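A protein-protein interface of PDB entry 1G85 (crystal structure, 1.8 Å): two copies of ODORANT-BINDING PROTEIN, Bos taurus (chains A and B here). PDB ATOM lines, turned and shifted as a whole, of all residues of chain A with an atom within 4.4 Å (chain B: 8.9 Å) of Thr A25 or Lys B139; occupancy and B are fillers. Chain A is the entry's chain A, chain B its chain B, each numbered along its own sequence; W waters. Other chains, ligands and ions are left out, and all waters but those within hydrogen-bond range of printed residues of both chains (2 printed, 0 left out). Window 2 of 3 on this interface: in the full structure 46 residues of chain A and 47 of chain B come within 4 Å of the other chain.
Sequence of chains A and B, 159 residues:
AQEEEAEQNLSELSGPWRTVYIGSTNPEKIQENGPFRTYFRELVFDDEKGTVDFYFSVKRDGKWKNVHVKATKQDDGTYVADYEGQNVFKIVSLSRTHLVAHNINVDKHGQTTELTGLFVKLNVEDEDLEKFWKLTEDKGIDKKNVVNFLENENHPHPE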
ATOM      1  N   SER A  24       6.933  18.245   3.635  1.00  0.00           N
ATOM      2  CA  SER A  24       8.378  18.310   3.434  1.00  0.00           C
ATOM      3  C   SER A  24       8.868  17.605   2.171  1.00  0.00           C
ATOM      4  O   SER A  24       8.340  16.558   1.791  1.00  0.00           O
ATOM      5  CB  SER A  24       9.082  17.708   4.656  1.00  0.00           C
ATOM      6  OG  SER A  24      10.489  17.796   4.546  1.00  0.00           O
ATOM      7  N   THR A  25       9.876  18.183   1.518  1.00  0.00           N
ATOM      8  CA  THR A  25      10.437  17.573   0.312  1.00  0.00           C
ATOM      9  C   THR A  25      11.251  16.343   0.718  1.00  0.00           C
ATOM     10  O   THR A  25      11.554  15.483  -0.110  1.00  0.00           O
ATOM     11  CB  THR A  25      11.349  18.551  -0.466  1.00  0.00           C
ATOM     12  OG1 THR A  25      12.347  19.089   0.412  1.00  0.00           O
ATOM     13  CG2 THR A  25      10.527  19.689  -1.063  1.00  0.00           C
ATOM     14  N   ASN A  26      11.603  16.274   1.997  1.00  0.00           N
ATOM     15  CA  ASN A  26      12.350  15.142   2.548  1.00  0.00           C
ATOM     16  C   ASN A  26      11.509  14.572   3.695  1.00  0.00           C
ATOM     17  O   ASN A  26      11.519  15.104   4.803  1.00  0.00           O
ATOM     18  CB  ASN A  26      13.702  15.603   3.097  1.00  0.00           C
ATOM     19  CG  ASN A  26      14.578  14.441   3.532  1.00  0.00           C
ATOM     20  OD1 ASN A  26      14.086  13.426   4.034  1.00  0.00           O
ATOM     21  ND2 ASN A  26      15.887  14.588   3.353  1.00  0.00           N
ATOM     22  N   PRO A  27      10.786  13.467   3.449  1.00  0.00           N
ATOM     23  CA  PRO A  27       9.943  12.861   4.487  1.00  0.00           C
ATOM     24  C   PRO A  27      10.618  12.533   5.820  1.00  0.00           C
ATOM     25  O   PRO A  27       9.992  12.630   6.872  1.00  0.00           O
ATOM     26  CB  PRO A  27       9.374  11.622   3.788  1.00  0.00           C
ATOM     27  CG  PRO A  27      10.449  11.256   2.817  1.00  0.00           C
ATOM     28  CD  PRO A  27      10.858  12.599   2.259  1.00  0.00           C
ATOM     29  N   HIS A 102       6.554  28.980   4.529  1.00  0.00           N
ATOM     30  CA  HIS A 102       7.468  28.194   3.722  1.00  0.00           C
ATOM     31  C   HIS A 102       8.841  28.322   4.380  1.00  0.00           C
ATOM     32  O   HIS A 102       9.308  29.436   4.630  1.00  0.00           O
ATOM     33  CB  HIS A 102       7.510  28.771   2.305  1.00  0.00           C
ATOM     34  CG  HIS A 102       8.606  28.217   1.449  1.00  0.00           C
ATOM     35  ND1 HIS A 102       9.136  28.915   0.386  1.00  0.00           N
ATOM     36  CD2 HIS A 102       9.259  27.032   1.486  1.00  0.00           C
ATOM     37  CE1 HIS A 102      10.070  28.182  -0.197  1.00  0.00           C
ATOM     38  NE2 HIS A 102      10.163  27.036   0.451  1.00  0.00           N
ATOM     39  N   THR A 113      16.238  21.135   2.474  1.00  0.00           N
ATOM     40  CA  THR A 113      14.887  20.610   2.644  1.00  0.00           C
ATOM     41  C   THR A 113      13.907  21.771   2.650  1.00  0.00           C
ATOM     42  O   THR A 113      14.118  22.750   3.363  1.00  0.00           O
ATOM     43  CB  THR A 113      14.724  19.865   3.985  1.00  0.00           C
ATOM     44  OG1 THR A 113      15.658  18.781   4.062  1.00  0.00           O
ATOM     45  CG2 THR A 113      13.303  19.314   4.117  1.00  0.00           C
ATOM     46  N   GLU A 114      12.851  21.682   1.847  1.00  0.00           N
ATOM     47  CA  GLU A 114      11.848  22.739   1.836  1.00  0.00           C
ATOM     48  C   GLU A 114      10.609  22.215   2.553  1.00  0.00           C
ATOM     49  O   GLU A 114      10.167  21.091   2.315  1.00  0.00           O
ATOM     50  CB  GLU A 114      11.501  23.160   0.408  1.00  0.00           C
ATOM     51  CG  GLU A 114      12.718  23.636  -0.395  1.00  0.00           C
ATOM     52  CD  GLU A 114      12.364  24.642  -1.469  1.00  0.00           C
ATOM     53  OE1 GLU A 114      13.077  24.692  -2.493  1.00  0.00           O
ATOM     54  OE2 GLU A 114      11.386  25.396  -1.291  1.00  0.00           O
ATOM     55  N   THR A 116       6.555  23.217   4.175  1.00  0.00           N
ATOM     56  CA  THR A 116       5.405  24.106   4.118  1.00  0.00           C
ATOM     57  C   THR A 116       4.615  23.817   5.382  1.00  0.00           C
ATOM     58  O   THR A 116       4.681  22.714   5.922  1.00  0.00           O
ATOM     59  CB  THR A 116       4.504  23.827   2.904  1.00  0.00           C
ATOM     60  OG1 THR A 116       4.121  22.446   2.899  1.00  0.00           O
ATOM     61  CG2 THR A 116       5.225  24.178   1.617  1.00  0.00           C
ATOM     62  N   PHE B 132      -2.618  26.495   1.803  1.00  0.00           N
ATOM     63  CA  PHE B 132      -1.581  25.563   2.232  1.00  0.00           C
ATOM     64  C   PHE B 132      -1.312  24.500   1.172  1.00  0.00           C
ATOM     65  O   PHE B 132      -0.164  24.213   0.852  1.00  0.00           O
ATOM     66  CB  PHE B 132      -1.971  24.857   3.535  1.00  0.00           C
ATOM     67  CG  PHE B 132      -1.092  23.681   3.856  1.00  0.00           C
ATOM     68  CD1 PHE B 132       0.220  23.870   4.293  1.00  0.00           C
ATOM     69  CD2 PHE B 132      -1.553  22.383   3.656  1.00  0.00           C
ATOM     70  CE1 PHE B 132       1.062  22.776   4.522  1.00  0.00           C
ATOM     71  CE2 PHE B 132      -0.721  21.280   3.881  1.00  0.00           C
ATOM     72  CZ  PHE B 132       0.589  21.476   4.315  1.00  0.00           C
ATOM     73  N   TRP B 133      -2.370  23.903   0.630  1.00  0.00           N
ATOM     74  CA  TRP B 133      -2.174  22.872  -0.374  1.00  0.00           C
ATOM     75  C   TRP B 133      -1.565  23.402  -1.671  1.00  0.00           C
ATOM     76  O   TRP B 133      -0.780  22.705  -2.308  1.00  0.00           O
ATOM     77  CB  TRP B 133      -3.483  22.131  -0.645  1.00  0.00           C
ATOM     78  CG  TRP B 133      -3.840  21.176   0.463  1.00  0.00           C
ATOM     79  CD1 TRP B 133      -4.892  21.275   1.327  1.00  0.00           C
ATOM     80  CD2 TRP B 133      -3.122  19.992   0.838  1.00  0.00           C
ATOM     81  NE1 TRP B 133      -4.874  20.227   2.218  1.00  0.00           N
ATOM     82  CE2 TRP B 133      -3.800  19.427   1.943  1.00  0.00           C
ATOM     83  CE3 TRP B 133      -1.974  19.360   0.353  1.00  0.00           C
ATOM     84  CZ2 TRP B 133      -3.364  18.249   2.566  1.00  0.00           C
ATOM     85  CZ3 TRP B 133      -1.540  18.187   0.974  1.00  0.00           C
ATOM     86  CH2 TRP B 133      -2.238  17.649   2.070  1.00  0.00           C
ATOM     87  N   LYS B 134      -1.911  24.630  -2.049  1.00  0.00           N
ATOM     88  CA  LYS B 134      -1.364  25.239  -3.267  1.00  0.00           C
ATOM     89  C   LYS B 134       0.138  25.460  -3.095  1.00  0.00           C
ATOM     90  O   LYS B 134       0.935  25.132  -3.979  1.00  0.00           O
ATOM     91  CB  LYS B 134      -2.064  26.578  -3.542  1.00  0.00           C
ATOM     92  CG  LYS B 134      -1.581  27.387  -4.818  1.00  0.00           C
ATOM     93  CD  LYS B 134      -1.541  26.524  -6.077  1.00  0.00           C
ATOM     94  CE  LYS B 134      -1.098  27.341  -7.349  1.00  0.00           C
ATOM     95  NZ  LYS B 134       0.165  28.117  -7.214  1.00  0.00           N
ATOM     96  N   LEU B 135       0.524  26.015  -1.948  1.00  0.00           N
ATOM     97  CA  LEU B 135       1.932  26.262  -1.662  1.00  0.00           C
ATOM     98  C   LEU B 135       2.688  24.943  -1.625  1.00  0.00           C
ATOM     99  O   LEU B 135       3.829  24.845  -2.079  1.00  0.00           O
ATOM    100  CB  LEU B 135       2.089  26.967  -0.306  1.00  0.00           C
ATOM    101  CG  LEU B 135       3.518  27.134   0.225  1.00  0.00           C
ATOM    102  CD1 LEU B 135       4.305  28.067  -0.687  1.00  0.00           C
ATOM    103  CD2 LEU B 135       3.478  27.688   1.648  1.00  0.00           C
ATOM    104  N   THR B 136       2.046  23.923  -1.069  1.00  0.00           N
ATOM    105  CA  THR B 136       2.672  22.620  -0.961  1.00  0.00           C
ATOM    106  C   THR B 136       2.930  22.020  -2.341  1.00  0.00           C
ATOM    107  O   THR B 136       3.993  21.455  -2.593  1.00  0.00           O
ATOM    108  CB  THR B 136       1.800  21.665  -0.107  1.00  0.00           C
ATOM    109  OG1 THR B 136       1.645  22.222   1.205  1.00  0.00           O
ATOM    110  CG2 THR B 136       2.449  20.291   0.002  1.00  0.00           C
ATOM    111  N   GLU B 137       1.969  22.154  -3.247  1.00  0.00           N
ATOM    112  CA  GLU B 137       2.182  21.602  -4.571  1.00  0.00           C
ATOM    113  C   GLU B 137       3.135  22.475  -5.383  1.00  0.00           C
ATOM    114  O   GLU B 137       3.827  21.973  -6.268  1.00  0.00           O
ATOM    115  CB  GLU B 137       0.848  21.383  -5.292  1.00  0.00           C
ATOM    116  CG  GLU B 137      -0.043  22.545  -5.394  1.00  0.00           C
ATOM    117  CD  GLU B 137      -1.480  22.120  -5.641  1.00  0.00           C
ATOM    118  OE1 GLU B 137      -2.293  22.969  -6.058  1.00  0.00           O
ATOM    119  OE2 GLU B 137      -1.793  20.932  -5.404  1.00  0.00           O
ATOM    120  N   ASP B 138       3.191  23.770  -5.066  1.00  0.00           N
ATOM    121  CA  ASP B 138       4.104  24.678  -5.763  1.00  0.00           C
ATOM    122  C   ASP B 138       5.537  24.232  -5.482  1.00  0.00           C
ATOM    123  O   ASP B 138       6.417  24.359  -6.332  1.00  0.00           O
ATOM    124  CB  ASP B 138       3.961  26.132  -5.268  1.00  0.00           C
ATOM    125  CG  ASP B 138       2.776  26.861  -5.880  1.00  0.00           C
ATOM    126  OD1 ASP B 138       2.216  26.372  -6.877  1.00  0.00           O
ATOM    127  OD2 ASP B 138       2.415  27.939  -5.363  1.00  0.00           O
ATOM    128  N   LYS B 139       5.767  23.713  -4.280  1.00  0.00           N
ATOM    129  CA  LYS B 139       7.105  23.286  -3.894  1.00  0.00           C
ATOM    130  C   LYS B 139       7.436  21.841  -4.248  1.00  0.00           C
ATOM    131  O   LYS B 139       8.463  21.313  -3.827  1.00  0.00           O
ATOM    132  CB  LYS B 139       7.311  23.535  -2.399  1.00  0.00           C
ATOM    133  CG  LYS B 139       7.075  24.992  -2.004  1.00  0.00           C
ATOM    134  CD  LYS B 139       7.872  25.936  -2.928  1.00  0.00           C
ATOM    135  CE  LYS B 139       7.666  27.388  -2.581  1.00  0.00           C
ATOM    136  NZ  LYS B 139       8.507  28.252  -3.459  1.00  0.00           N
ATOM    137  N   GLY B 140       6.570  21.209  -5.030  1.00  0.00           N
ATOM    138  CA  GLY B 140       6.813  19.836  -5.438  1.00  0.00           C
ATOM    139  C   GLY B 140       6.787  18.810  -4.321  1.00  0.00           C
ATOM    140  O   GLY B 140       7.480  17.789  -4.392  1.00  0.00           O
ATOM    141  N   ILE B 141       5.999  19.084  -3.286  1.00  0.00           N
ATOM    142  CA  ILE B 141       5.865  18.180  -2.146  1.00  0.00           C
ATOM    143  C   ILE B 141       4.702  17.218  -2.363  1.00  0.00           C
ATOM    144  O   ILE B 141       3.571  17.636  -2.607  1.00  0.00           O
ATOM    145  CB  ILE B 141       5.641  18.972  -0.833  1.00  0.00           C
ATOM    146  CG1 ILE B 141       6.897  19.780  -0.509  1.00  0.00           C
ATOM    147  CG2 ILE B 141       5.299  18.023   0.322  1.00  0.00           C
ATOM    148  CD1 ILE B 141       6.737  20.748   0.648  1.00  0.00           C
ATOM    149  N   ASP B 142       4.996  15.924  -2.283  1.00  0.00           N
ATOM    150  CA  ASP B 142       3.988  14.884  -2.459  1.00  0.00           C
ATOM    151  C   ASP B 142       3.038  14.888  -1.262  1.00  0.00           C
ATOM    152  O   ASP B 142       3.468  15.069  -0.124  1.00  0.00           O
ATOM    153  CB  ASP B 142       4.670  13.518  -2.574  1.00  0.00           C
ATOM    154  CG  ASP B 142       3.748  12.443  -3.125  1.00  0.00           C
ATOM    155  OD1 ASP B 142       2.676  12.201  -2.530  1.00  0.00           O
ATOM    156  OD2 ASP B 142       4.102  11.835  -4.157  1.00  0.00           O
ATOM    157  N   LYS B 144       1.675  12.552   0.261  1.00  0.00           N
ATOM    158  CA  LYS B 144       1.953  11.524   1.251  1.00  0.00           C
ATOM    159  C   LYS B 144       3.121  11.919   2.149  1.00  0.00           C
ATOM    160  O   LYS B 144       3.464  11.212   3.096  1.00  0.00           O
ATOM    161  CB  LYS B 144       2.202  10.168   0.573  1.00  0.00           C
ATOM    162  CG  LYS B 144       3.358  10.075  -0.464  1.00  0.00           C
ATOM    163  CD  LYS B 144       4.732  10.049   0.199  1.00  0.00           C
ATOM    164  CE  LYS B 144       5.873   9.926  -0.844  1.00  0.00           C
ATOM    165  NZ  LYS B 144       5.749  10.853  -1.998  1.00  0.00           N
ATOM    166  N   ASN B 145       3.717  13.069   1.849  1.00  0.00           N
ATOM    167  CA  ASN B 145       4.831  13.588   2.629  1.00  0.00           C
ATOM    168  C   ASN B 145       4.350  14.756   3.488  1.00  0.00           C
ATOM    169  O   ASN B 145       5.092  15.697   3.757  1.00  0.00           O
ATOM    170  CB  ASN B 145       5.961  14.031   1.698  1.00  0.00           C
ATOM    171  CG  ASN B 145       6.729  12.851   1.120  1.00  0.00           C
ATOM    172  OD1 ASN B 145       7.484  12.993   0.160  1.00  0.00           O
ATOM    173  ND2 ASN B 145       6.546  11.677   1.718  1.00  0.00           N
ATOM    174  N   VAL B 146       3.089  14.681   3.901  1.00  0.00           N
ATOM    175  CA  VAL B 146       2.480  15.704   4.749  1.00  0.00           C
ATOM    176  C   VAL B 146       1.892  15.030   5.989  1.00  0.00           C
ATOM    177  O   VAL B 146       1.222  14.001   5.891  1.00  0.00           O
ATOM    178  CB  VAL B 146       1.352  16.449   4.009  1.00  0.00           C
ATOM    179  CG1 VAL B 146       0.705  17.470   4.936  1.00  0.00           C
ATOM    180  CG2 VAL B 146       1.914  17.122   2.756  1.00  0.00           C
HETATM  181  O   HOH W   1      11.309  27.446  -3.103  1.00  0.00           O
HETATM  182  O   HOH W   2       8.084  15.340  -0.571  1.00  0.00           O
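Of the 8 printed residues of chain A, 6 touch a printed residue of chain B. Printed residues of chain A that touch a printed residue of chain B: Ser A24, Thr A25, Pro A27, His A102, Glu A114 and Thr A116. Hydrophobic or aromatic side chains of chain A within 4 Å of the printed part of chain B: Pro A27 and His A102. Among the printed residues, 12 pairs touch across the chains. Among the printed residues, no Asp or Glu carboxylate lies within 4 Å of a Lys or Arg side-chain nitrogen of the other chain.
No position is printed for both chains. Of the 12 pairs that touch across the chains among the printed residues, none has its exchanged pair printed and touching as well.
The side-chain hydroxyl (OG) of Ser A24 is in hydrogen-bond range of the backbone carbonyl oxygen (O) of Asn A26 (2.9 Å). The side-chain hydroxyl (OG1) of Thr A25 is in hydrogen-bond range of the backbone NH (N) of Glu A114. The side-chain carboxylate (OE2) of Glu A114 is in hydrogen-bond range of a ring nitrogen (NE2) of His A102, at 2.7 Å. OG1 of Thr B136 is in hydrogen-bond range of O of Phe B132 (2.7 Å). The backbone NH of Ile B141 sits at hydrogen-bond distance from the backbone carbonyl oxygen of Thr B136.
The backbone carbonyl oxygen (O) of Asn B145 lies within hydrogen-bond range of the backbone NH (N) of Ser A24 (3.1 Å). The side-chain hydroxyl (OG1) of Thr A116 lies within hydrogen-bond range of the side-chain hydroxyl (OG1) of Thr B136 (3.0 Å).
Water W2 bridges OD1 of Asn B145 and O of Ser A24. Water W1 bridges the side-chain carboxylate of Glu A114 (2.7 Å) and the side-chain amino group of Lys B139 (2.9 Å).
Lys B139 touches just these residues of chain A: Thr A25 (3.8 Å), His A102 (3.5 Å) and Glu A114 (3.9 Å). Ser A24 touches just these residues of chain B: Ile B141 and Asn B145. Of the printed residues of chain B, Pro A27 touches Asn B145. Of the printed residues of chain A, Phe B132 touches Thr A116 (3.5 Å). Asn A26 touches none of the printed residues of chain B. The nearest residue of chain B that does not touch Thr A25 is Asn B145 (4.8 Å). The nearest residue of chain A that does not touch Lys B139 is Thr A116 (4.1 Å). The nearest printed residue of chain A that does not touch Ile B141 is Asn A26 (6.4 Å).
Among the printed residues, merely in contact across the chains: Ser A24 with Ile B141, Thr A25 with Lys B139, Thr A25 with Ile B141, Pro A27 with Asn B145, His A102 with Lys B139, Glu A114 with Lys B139, Glu A114 with Ile B141, Thr A116 with Phe B132, Thr A116 with Leu B135 and Thr A116 with Ile B141.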
